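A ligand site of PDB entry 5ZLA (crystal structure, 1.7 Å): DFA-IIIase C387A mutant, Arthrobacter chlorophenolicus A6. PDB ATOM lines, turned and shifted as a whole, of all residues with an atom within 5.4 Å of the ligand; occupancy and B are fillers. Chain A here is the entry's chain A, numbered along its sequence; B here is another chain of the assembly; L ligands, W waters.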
ATOM      1  N   PHE A  80      -2.075  22.088 -22.573  1.00  0.00           N
ATOM      2  CA  PHE A  80      -2.863  21.155 -23.355  1.00  0.00           C
ATOM      3  C   PHE A  80      -2.255  20.871 -24.720  1.00  0.00           C
ATOM      4  O   PHE A  80      -1.838  21.793 -25.426  1.00  0.00           O
ATOM      5  CB  PHE A  80      -4.316  21.649 -23.542  1.00  0.00           C
ATOM      6  CG  PHE A  80      -5.158  20.692 -24.327  1.00  0.00           C
ATOM      7  CD1 PHE A  80      -5.843  19.665 -23.686  1.00  0.00           C
ATOM      8  CD2 PHE A  80      -5.229  20.780 -25.713  1.00  0.00           C
ATOM      9  CE1 PHE A  80      -6.569  18.732 -24.424  1.00  0.00           C
ATOM     10  CE2 PHE A  80      -5.962  19.869 -26.451  1.00  0.00           C
ATOM     11  CZ  PHE A  80      -6.648  18.851 -25.800  1.00  0.00           C
ATOM     12  N   SER A  82      -3.401  17.721 -27.911  1.00  0.00           N
ATOM     13  CA  SER A  82      -4.382  16.652 -28.168  1.00  0.00           C
ATOM     14  C   SER A  82      -3.728  15.284 -28.159  1.00  0.00           C
ATOM     15  O   SER A  82      -3.279  14.802 -29.189  1.00  0.00           O
ATOM     16  CB  SER A  82      -5.132  16.854 -29.494  1.00  0.00           C
ATOM     17  OG  SER A  82      -6.067  15.784 -29.680  1.00  0.00           O
ATOM     18  N   SER A  84      -5.396  12.700 -27.870  1.00  0.00           N
ATOM     19  CA  SER A  84      -6.321  11.927 -28.686  1.00  0.00           C
ATOM     20  C   SER A  84      -5.854  11.879 -30.164  1.00  0.00           C
ATOM     21  O   SER A  84      -5.751  10.801 -30.765  1.00  0.00           O
ATOM     22  CB  SER A  84      -7.734  12.515 -28.572  1.00  0.00           C
ATOM     23  OG  SER A  84      -8.655  11.824 -29.404  1.00  0.00           O
ATOM     24  N   ILE A  85      -5.530  13.033 -30.725  1.00  0.00           N
ATOM     25  CA  ILE A  85      -5.003  13.071 -32.093  1.00  0.00           C
ATOM     26  C   ILE A  85      -3.702  12.260 -32.160  1.00  0.00           C
ATOM     27  O   ILE A  85      -3.552  11.408 -33.038  1.00  0.00           O
ATOM     28  CB  ILE A  85      -4.820  14.519 -32.590  1.00  0.00           C
ATOM     29  CG1 ILE A  85      -6.199  15.131 -32.857  1.00  0.00           C
ATOM     30  CG2 ILE A  85      -3.945  14.560 -33.850  1.00  0.00           C
ATOM     31  CD1 ILE A  85      -6.237  16.627 -33.113  1.00  0.00           C
ATOM     32  N   TYR A 163     -11.799   6.556 -23.139  1.00  0.00           N
ATOM     33  CA  TYR A 163     -12.078   7.530 -22.068  1.00  0.00           C
ATOM     34  C   TYR A 163     -12.175   6.885 -20.674  1.00  0.00           C
ATOM     35  O   TYR A 163     -12.752   7.470 -19.749  1.00  0.00           O
ATOM     36  CB  TYR A 163     -13.328   8.381 -22.357  1.00  0.00           C
ATOM     37  CG  TYR A 163     -13.202   9.347 -23.504  1.00  0.00           C
ATOM     38  CD1 TYR A 163     -13.434   8.954 -24.815  1.00  0.00           C
ATOM     39  CD2 TYR A 163     -12.880  10.687 -23.278  1.00  0.00           C
ATOM     40  CE1 TYR A 163     -13.346   9.858 -25.871  1.00  0.00           C
ATOM     41  CE2 TYR A 163     -12.795  11.599 -24.314  1.00  0.00           C
ATOM     42  CZ  TYR A 163     -13.032  11.186 -25.616  1.00  0.00           C
ATOM     43  OH  TYR A 163     -12.967  12.072 -26.668  1.00  0.00           O
ATOM     44  N   PHE A 207      -9.509  25.017 -19.564  1.00  0.00           N
ATOM     45  CA  PHE A 207      -9.514  24.186 -20.763  1.00  0.00           C
ATOM     46  C   PHE A 207      -9.610  22.749 -20.277  1.00  0.00           C
ATOM     47  O   PHE A 207      -8.674  22.215 -19.684  1.00  0.00           O
ATOM     48  CB  PHE A 207      -8.234  24.411 -21.586  1.00  0.00           C
ATOM     49  CG  PHE A 207      -8.335  23.919 -22.995  1.00  0.00           C
ATOM     50  CD1 PHE A 207      -8.132  22.566 -23.321  1.00  0.00           C
ATOM     51  CD2 PHE A 207      -8.664  24.818 -24.031  1.00  0.00           C
ATOM     52  CE1 PHE A 207      -8.257  22.130 -24.630  1.00  0.00           C
ATOM     53  CE2 PHE A 207      -8.773  24.369 -25.327  1.00  0.00           C
ATOM     54  CZ  PHE A 207      -8.562  23.035 -25.630  1.00  0.00           C
ATOM     55  N   ALA A 209     -10.594  19.119 -21.547  1.00  0.00           N
ATOM     56  CA  ALA A 209     -10.880  18.434 -22.790  1.00  0.00           C
ATOM     57  C   ALA A 209     -10.273  17.047 -22.854  1.00  0.00           C
ATOM     58  O   ALA A 209      -9.253  16.762 -22.210  1.00  0.00           O
ATOM     59  CB  ALA A 209     -10.403  19.281 -23.958  1.00  0.00           C
ATOM     60  N   GLU A 210     -10.878  16.197 -23.674  1.00  0.00           N
ATOM     61  CA  GLU A 210     -10.401  14.822 -23.847  1.00  0.00           C
ATOM     62  C   GLU A 210     -10.367  14.095 -22.489  1.00  0.00           C
ATOM     63  O   GLU A 210      -9.426  13.359 -22.182  1.00  0.00           O
ATOM     64  CB  GLU A 210      -9.061  14.802 -24.576  1.00  0.00           C
ATOM     65  CG  GLU A 210      -9.178  15.409 -25.958  1.00  0.00           C
ATOM     66  CD  GLU A 210      -7.908  15.413 -26.773  1.00  0.00           C
ATOM     67  OE1 GLU A 210      -6.899  14.784 -26.384  1.00  0.00           O
ATOM     68  OE2 GLU A 210      -7.929  16.069 -27.855  1.00  0.00           O
ATOM     69  N   GLY A 232     -14.628  19.741 -23.602  1.00  0.00           N
ATOM     70  CA  GLY A 232     -15.003  18.615 -24.456  1.00  0.00           C
ATOM     71  C   GLY A 232     -14.802  17.290 -23.755  1.00  0.00           C
ATOM     72  O   GLY A 232     -13.689  16.960 -23.329  1.00  0.00           O
ATOM     73  N   ALA A 233     -15.874  16.518 -23.650  1.00  0.00           N
ATOM     74  CA  ALA A 233     -15.880  15.283 -22.889  1.00  0.00           C
ATOM     75  C   ALA A 233     -15.913  14.051 -23.815  1.00  0.00           C
ATOM     76  O   ALA A 233     -15.562  14.147 -25.004  1.00  0.00           O
ATOM     77  CB  ALA A 233     -17.037  15.314 -21.903  1.00  0.00           C
ATOM     78  N   PHE A 256     -17.552  21.830 -26.902  1.00  0.00           N
ATOM     79  CA  PHE A 256     -17.386  21.114 -28.150  1.00  0.00           C
ATOM     80  C   PHE A 256     -17.512  19.623 -27.847  1.00  0.00           C
ATOM     81  O   PHE A 256     -17.626  19.240 -26.691  1.00  0.00           O
ATOM     82  CB  PHE A 256     -16.070  21.498 -28.855  1.00  0.00           C
ATOM     83  CG  PHE A 256     -14.870  21.516 -27.952  1.00  0.00           C
ATOM     84  CD1 PHE A 256     -14.186  20.348 -27.670  1.00  0.00           C
ATOM     85  CD2 PHE A 256     -14.397  22.715 -27.412  1.00  0.00           C
ATOM     86  CE1 PHE A 256     -13.061  20.361 -26.856  1.00  0.00           C
ATOM     87  CE2 PHE A 256     -13.291  22.731 -26.601  1.00  0.00           C
ATOM     88  CZ  PHE A 256     -12.620  21.553 -26.313  1.00  0.00           C
ATOM     89  N   PRO A 257     -17.574  18.776 -28.885  1.00  0.00           N
ATOM     90  CA  PRO A 257     -17.796  17.341 -28.632  1.00  0.00           C
ATOM     91  C   PRO A 257     -16.641  16.686 -27.832  1.00  0.00           C
ATOM     92  O   PRO A 257     -15.593  17.291 -27.684  1.00  0.00           O
ATOM     93  CB  PRO A 257     -17.935  16.763 -30.054  1.00  0.00           C
ATOM     94  CG  PRO A 257     -18.457  17.920 -30.854  1.00  0.00           C
ATOM     95  CD  PRO A 257     -17.687  19.095 -30.320  1.00  0.00           C
ATOM     96  N   ARG A 258     -16.813  15.476 -27.291  1.00  0.00           N
ATOM     97  CA  ARG A 258     -17.896  14.544 -27.616  1.00  0.00           C
ATOM     98  C   ARG A 258     -18.535  13.912 -26.372  1.00  0.00           C
ATOM     99  O   ARG A 258     -18.779  12.704 -26.308  1.00  0.00           O
ATOM    100  CB  ARG A 258     -17.381  13.485 -28.586  1.00  0.00           C
ATOM    101  CG  ARG A 258     -16.150  12.714 -28.113  1.00  0.00           C
ATOM    102  CD  ARG A 258     -15.764  11.600 -29.095  1.00  0.00           C
ATOM    103  NE  ARG A 258     -15.296  12.161 -30.349  1.00  0.00           N
ATOM    104  CZ  ARG A 258     -14.091  12.702 -30.538  1.00  0.00           C
ATOM    105  NH1 ARG A 258     -13.202  12.762 -29.559  1.00  0.00           N
ATOM    106  NH2 ARG A 258     -13.777  13.207 -31.737  1.00  0.00           N
ATOM    107  N   PHE A 281     -22.182  15.844 -31.244  1.00  0.00           N
ATOM    108  CA  PHE A 281     -22.317  14.857 -32.315  1.00  0.00           C
ATOM    109  C   PHE A 281     -23.488  13.906 -32.096  1.00  0.00           C
ATOM    110  O   PHE A 281     -23.707  12.979 -32.885  1.00  0.00           O
ATOM    111  CB  PHE A 281     -21.020  14.052 -32.454  1.00  0.00           C
ATOM    112  CG  PHE A 281     -19.829  14.849 -32.952  1.00  0.00           C
ATOM    113  CD1 PHE A 281     -19.946  15.869 -33.895  1.00  0.00           C
ATOM    114  CD2 PHE A 281     -18.543  14.508 -32.519  1.00  0.00           C
ATOM    115  CE1 PHE A 281     -18.808  16.548 -34.359  1.00  0.00           C
ATOM    116  CE2 PHE A 281     -17.418  15.189 -32.976  1.00  0.00           C
ATOM    117  CZ  PHE A 281     -17.559  16.220 -33.892  1.00  0.00           C
ATOM    118  N   GLU A 307     -20.291  13.183 -36.117  1.00  0.00           N
ATOM    119  CA  GLU A 307     -18.846  13.004 -35.948  1.00  0.00           C
ATOM    120  C   GLU A 307     -18.152  12.892 -37.317  1.00  0.00           C
ATOM    121  O   GLU A 307     -18.553  12.048 -38.122  1.00  0.00           O
ATOM    122  CB  GLU A 307     -18.574  11.735 -35.157  1.00  0.00           C
ATOM    123  CG  GLU A 307     -17.112  11.308 -35.068  1.00  0.00           C
ATOM    124  CD  GLU A 307     -16.275  12.208 -34.194  1.00  0.00           C
ATOM    125  OE1 GLU A 307     -16.438  12.148 -32.951  1.00  0.00           O
ATOM    126  OE2 GLU A 307     -15.448  12.942 -34.766  1.00  0.00           O
ATOM    127  N   TRP A 309     -14.653  12.456 -37.688  1.00  0.00           N
ATOM    128  CA  TRP A 309     -13.337  11.870 -37.547  1.00  0.00           C
ATOM    129  C   TRP A 309     -13.467  10.359 -37.379  1.00  0.00           C
ATOM    130  O   TRP A 309     -14.141   9.876 -36.464  1.00  0.00           O
ATOM    131  CB  TRP A 309     -12.626  12.509 -36.344  1.00  0.00           C
ATOM    132  CG  TRP A 309     -11.182  12.172 -36.213  1.00  0.00           C
ATOM    133  CD1 TRP A 309     -10.258  12.006 -37.205  1.00  0.00           C
ATOM    134  CD2 TRP A 309     -10.481  11.983 -34.990  1.00  0.00           C
ATOM    135  NE1 TRP A 309      -9.019  11.724 -36.667  1.00  0.00           N
ATOM    136  CE2 TRP A 309      -9.142  11.690 -35.301  1.00  0.00           C
ATOM    137  CE3 TRP A 309     -10.871  12.021 -33.639  1.00  0.00           C
ATOM    138  CZ2 TRP A 309      -8.181  11.438 -34.320  1.00  0.00           C
ATOM    139  CZ3 TRP A 309      -9.917  11.771 -32.670  1.00  0.00           C
ATOM    140  CH2 TRP A 309      -8.591  11.501 -33.003  1.00  0.00           C
ATOM    141  N   PHE A 312     -13.872   7.804 -34.184  1.00  0.00           N
ATOM    142  CA  PHE A 312     -15.115   7.861 -33.411  1.00  0.00           C
ATOM    143  C   PHE A 312     -16.381   7.886 -34.265  1.00  0.00           C
ATOM    144  O   PHE A 312     -17.475   8.115 -33.739  1.00  0.00           O
ATOM    145  CB  PHE A 312     -15.071   9.081 -32.494  1.00  0.00           C
ATOM    146  CG  PHE A 312     -14.070   8.956 -31.375  1.00  0.00           C
ATOM    147  CD1 PHE A 312     -14.380   8.243 -30.226  1.00  0.00           C
ATOM    148  CD2 PHE A 312     -12.816   9.546 -31.479  1.00  0.00           C
ATOM    149  CE1 PHE A 312     -13.472   8.134 -29.199  1.00  0.00           C
ATOM    150  CE2 PHE A 312     -11.898   9.446 -30.439  1.00  0.00           C
ATOM    151  CZ  PHE A 312     -12.237   8.736 -29.297  1.00  0.00           C
ATOM    152  N   GLN A 391     -12.814  18.351 -38.964  1.00  0.00           N
ATOM    153  CA  GLN A 391     -13.623  19.102 -38.011  1.00  0.00           C
ATOM    154  C   GLN A 391     -13.990  20.503 -38.519  1.00  0.00           C
ATOM    155  O   GLN A 391     -15.153  20.896 -38.482  1.00  0.00           O
ATOM    156  CB  GLN A 391     -12.896  19.214 -36.675  1.00  0.00           C
ATOM    157  CG  GLN A 391     -12.745  17.902 -35.924  1.00  0.00           C
ATOM    158  CD  GLN A 391     -11.673  17.942 -34.843  1.00  0.00           C
ATOM    159  OE1 GLN A 391     -10.974  18.958 -34.651  1.00  0.00           O
ATOM    160  NE2 GLN A 391     -11.531  16.825 -34.125  1.00  0.00           N
ATOM    161  N   ARG B 134       0.189  20.579 -34.353  1.00  0.00           N
ATOM    162  CA  ARG B 134       0.035  22.022 -34.249  1.00  0.00           C
ATOM    163  C   ARG B 134       0.657  22.524 -32.959  1.00  0.00           C
ATOM    164  O   ARG B 134       0.514  21.889 -31.913  1.00  0.00           O
ATOM    165  CB  ARG B 134      -1.436  22.415 -34.269  1.00  0.00           C
ATOM    166  CG  ARG B 134      -2.092  22.194 -35.615  1.00  0.00           C
ATOM    167  CD  ARG B 134      -3.580  22.306 -35.489  1.00  0.00           C
ATOM    168  NE  ARG B 134      -4.117  21.227 -34.653  1.00  0.00           N
ATOM    169  CZ  ARG B 134      -5.372  21.169 -34.227  1.00  0.00           C
ATOM    170  NH1 ARG B 134      -6.232  22.148 -34.526  1.00  0.00           N
ATOM    171  NH2 ARG B 134      -5.780  20.143 -33.484  1.00  0.00           N
ATOM    172  N   ASP B 177      -3.491  25.375 -31.460  1.00  0.00           N
ATOM    173  CA  ASP B 177      -4.534  24.779 -30.622  1.00  0.00           C
ATOM    174  C   ASP B 177      -4.368  25.262 -29.189  1.00  0.00           C
ATOM    175  O   ASP B 177      -3.256  25.308 -28.673  1.00  0.00           O
ATOM    176  CB  ASP B 177      -4.424  23.256 -30.669  1.00  0.00           C
ATOM    177  CG  ASP B 177      -5.653  22.541 -30.134  1.00  0.00           C
ATOM    178  OD1 ASP B 177      -6.753  23.135 -30.033  1.00  0.00           O
ATOM    179  OD2 ASP B 177      -5.531  21.336 -29.856  1.00  0.00           O
ATOM    180  N   SER B 178      -5.466  25.625 -28.564  1.00  0.00           N
ATOM    181  CA  SER B 178      -5.513  25.901 -27.127  1.00  0.00           C
ATOM    182  C   SER B 178      -4.625  27.070 -26.711  1.00  0.00           C
ATOM    183  O   SER B 178      -4.086  27.081 -25.617  1.00  0.00           O
ATOM    184  CB  SER B 178      -5.151  24.630 -26.326  1.00  0.00           C
ATOM    185  OG  SER B 178      -5.605  24.726 -24.976  1.00  0.00           O
ATOM    186  N   ASP B 199      -7.567  27.083 -33.382  1.00  0.00           N
ATOM    187  CA  ASP B 199      -8.485  26.089 -32.833  1.00  0.00           C
ATOM    188  C   ASP B 199      -8.518  26.296 -31.313  1.00  0.00           C
ATOM    189  O   ASP B 199      -7.474  26.310 -30.649  1.00  0.00           O
ATOM    190  CB  ASP B 199      -8.011  24.689 -33.203  1.00  0.00           C
ATOM    191  CG  ASP B 199      -8.999  23.598 -32.868  1.00  0.00           C
ATOM    192  OD1 ASP B 199     -10.003  23.845 -32.177  1.00  0.00           O
ATOM    193  OD2 ASP B 199      -8.752  22.442 -33.328  1.00  0.00           O
ATOM    194  N   ALA B 200      -9.720  26.455 -30.762  1.00  0.00           N
ATOM    195  CA  ALA B 200      -9.930  26.436 -29.323  1.00  0.00           C
ATOM    196  C   ALA B 200      -9.068  27.487 -28.621  1.00  0.00           C
ATOM    197  O   ALA B 200      -8.488  27.244 -27.581  1.00  0.00           O
ATOM    198  CB  ALA B 200      -9.688  25.035 -28.760  1.00  0.00           C
ATOM    199  N   GLN B 222     -11.750  27.237 -35.554  1.00  0.00           N
ATOM    200  CA  GLN B 222     -12.877  26.613 -34.911  1.00  0.00           C
ATOM    201  C   GLN B 222     -12.831  26.701 -33.400  1.00  0.00           C
ATOM    202  O   GLN B 222     -11.759  26.807 -32.808  1.00  0.00           O
ATOM    203  CB  GLN B 222     -13.020  25.146 -35.329  1.00  0.00           C
ATOM    204  CG  GLN B 222     -11.873  24.239 -34.932  1.00  0.00           C
ATOM    205  CD  GLN B 222     -12.136  22.776 -35.223  1.00  0.00           C
ATOM    206  OE1 GLN B 222     -13.254  22.386 -35.581  1.00  0.00           O
ATOM    207  NE2 GLN B 222     -11.121  21.949 -35.026  1.00  0.00           N
ATOM    208  N   ALA B 223     -14.019  26.624 -32.816  1.00  0.00           N
ATOM    209  CA  ALA B 223     -14.192  26.399 -31.388  1.00  0.00           C
ATOM    210  C   ALA B 223     -13.488  27.415 -30.497  1.00  0.00           C
ATOM    211  O   ALA B 223     -13.056  27.065 -29.413  1.00  0.00           O
ATOM    212  CB  ALA B 223     -13.761  24.982 -31.041  1.00  0.00           C
HETATM  213  C1  LIG L   1     -11.052  16.500 -28.989  1.00  0.00           C
HETATM  214  C2  LIG L   1     -10.972  15.960 -30.453  1.00  0.00           C
HETATM  215  C3  LIG L   1     -12.487  17.061 -28.882  1.00  0.00           C
HETATM  216  C4  LIG L   1      -8.726  19.533 -29.285  1.00  0.00           C
HETATM  217  C5  LIG L   1      -9.393  17.714 -30.974  1.00  0.00           C
HETATM  218  C6  LIG L   1     -13.248  16.480 -30.103  1.00  0.00           C
HETATM  219  O1  LIG L   1     -10.524  16.966 -31.393  1.00  0.00           O
HETATM  220  C7  LIG L   1     -10.032  14.783 -30.597  1.00  0.00           C
HETATM  221  O2  LIG L   1     -10.510  13.736 -29.736  1.00  0.00           O
HETATM  222  O3  LIG L   1     -12.302  15.646 -30.834  1.00  0.00           O
HETATM  223  C8  LIG L   1     -13.808  17.587 -30.996  1.00  0.00           C
HETATM  224  O4  LIG L   1     -14.623  16.927 -32.018  1.00  0.00           O
HETATM  225  O5  LIG L   1     -13.071  16.682 -27.604  1.00  0.00           O
HETATM  226  O6  LIG L   1     -10.069  17.544 -28.661  1.00  0.00           O
HETATM  227  C9  LIG L   1      -9.786  18.519 -29.763  1.00  0.00           C
HETATM  228  O7  LIG L   1     -10.935  19.346 -30.153  1.00  0.00           O
HETATM  229  C10 LIG L   1     -10.765  20.631 -29.492  1.00  0.00           C
HETATM  230  C11 LIG L   1     -11.657  21.722 -30.049  1.00  0.00           C
HETATM  231  O8  LIG L   1     -11.505  21.726 -31.471  1.00  0.00           O
HETATM  232  C12 LIG L   1      -9.288  20.872 -29.737  1.00  0.00           C
HETATM  233  O9  LIG L   1      -8.804  21.866 -28.896  1.00  0.00           O
HETATM  234  O10 LIG L   1      -7.393  19.410 -29.846  1.00  0.00           O
HETATM  235  O   HOH W   1     -15.449  18.979 -33.541  1.00  0.00           O
HETATM  236  O   HOH W   2      -8.558  19.819 -33.234  1.00  0.00           O
HETATM  237  O   HOH W   3     -13.879  15.075 -34.103  1.00  0.00           O
HETATM  238  O   HOH W   4     -12.973  14.689 -25.870  1.00  0.00           O
HETATM  239  O   HOH W   5     -14.044  21.415 -33.034  1.00  0.00           O
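The backbone carbonyl oxygen (O) of Pro 257 sits at hydrogen-bond distance from an oxygen (O5) of the ligand (2.6 Å). An oxygen (O9) of the ligand lies within hydrogen-bond range of the side-chain carboxylate of Asp 177 of chain B, 2.7 Å away. OG of Ser 84 lies within hydrogen-bond range of O2 of the ligand, 2.7 Å away. An oxygen (O8) of the ligand is in hydrogen-bond range of the side-chain carboxylate (OD1) of Asp 199 of chain B, at 2.7 Å. O6 of the ligand lies close to OE2 of Glu 210, at 2.7 Å. NH1 of Arg 258 lies within hydrogen-bond range of O2 of the ligand (2.9 Å). NE2 of Gln 391 is in hydrogen-bond range of O1 of the ligand, at 2.9 Å.
The side-chain carboxylate (OD2) of Asp 177 of chain B lies within salt-bridge range of the guanidinium group (NH2) of Arg 134 of chain B, 3.8 Å away. The side-chain amide nitrogen (NE2) of Gln 222 of chain B is in hydrogen-bond range of the side-chain carboxylate (OD2) of Asp 199 of chain B (3.0 Å). The side-chain carboxylate of Asp 199 of chain B lies within salt-bridge range of the guanidinium group of Arg 134 of chain B (2.8 Å). The guanidinium group (NH1) of Arg 258 is in hydrogen-bond range of the side-chain hydroxyl (OH) of Tyr 163 (3.0 Å). The backbone NH of Arg 258 lies within hydrogen-bond range of the backbone carbonyl oxygen of Ala 233, 2.9 Å away. The side-chain carboxylate of Glu 307 lies within salt-bridge range of the guanidinium group of Arg 258 (2.8 Å). The side-chain amide nitrogen (NE2) of Gln 222 of chain B sits at hydrogen-bond distance from the side-chain amide oxygen (OE1) of Gln 391 (3.0 Å). OG of Ser 82 lies within hydrogen-bond range of N of Ile 85, 3.0 Å away.
Water W4 lies within hydrogen-bond range of O5 of the ligand (2.6 Å), OH of Tyr 163 (2.7 Å), O of Ala 233 (2.8 Å), N of Glu 210 (3.4 Å) and O of Gly 232 (3.5 Å). Water W3 lies within hydrogen-bond range of the side-chain carboxylate (OE2) of Glu 307 (2.7 Å), an oxygen (O4) of the ligand (2.9 Å), the side-chain amide nitrogen (NE2) of Gln 391 (2.9 Å) and the guanidinium group (NH2) of Arg 258 (3.0 Å). Water W5 lies within hydrogen-bond range of OE1 of Gln 222 of chain B (2.8 Å) and O8 of the ligand (3.0 Å). Water W2 lies within hydrogen-bond range of OD2 of Asp 199 of chain B, NH2 of Arg 134 of chain B and OE1 of Gln 391.
Residues that only touch the ligand: Ala 200 of chain B, Phe 281, Ser 82, Phe 207, Phe 256, Trp 309, Gln 222 of chain B, Phe 80, Ile 85 and Ala 223 of chain B. Within 4 Å of the ligand: Phe 80, Ser 82, Ser 84, Ile 85, Phe 207, Glu 210, Phe 256, Pro 257, Arg 258, Phe 281, Trp 309, Gln 391, Asp 177 of chain B, Asp 199 of chain B, Ala 200 of chain B, Gln 222 of chain B and Ala 223 of chain B.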
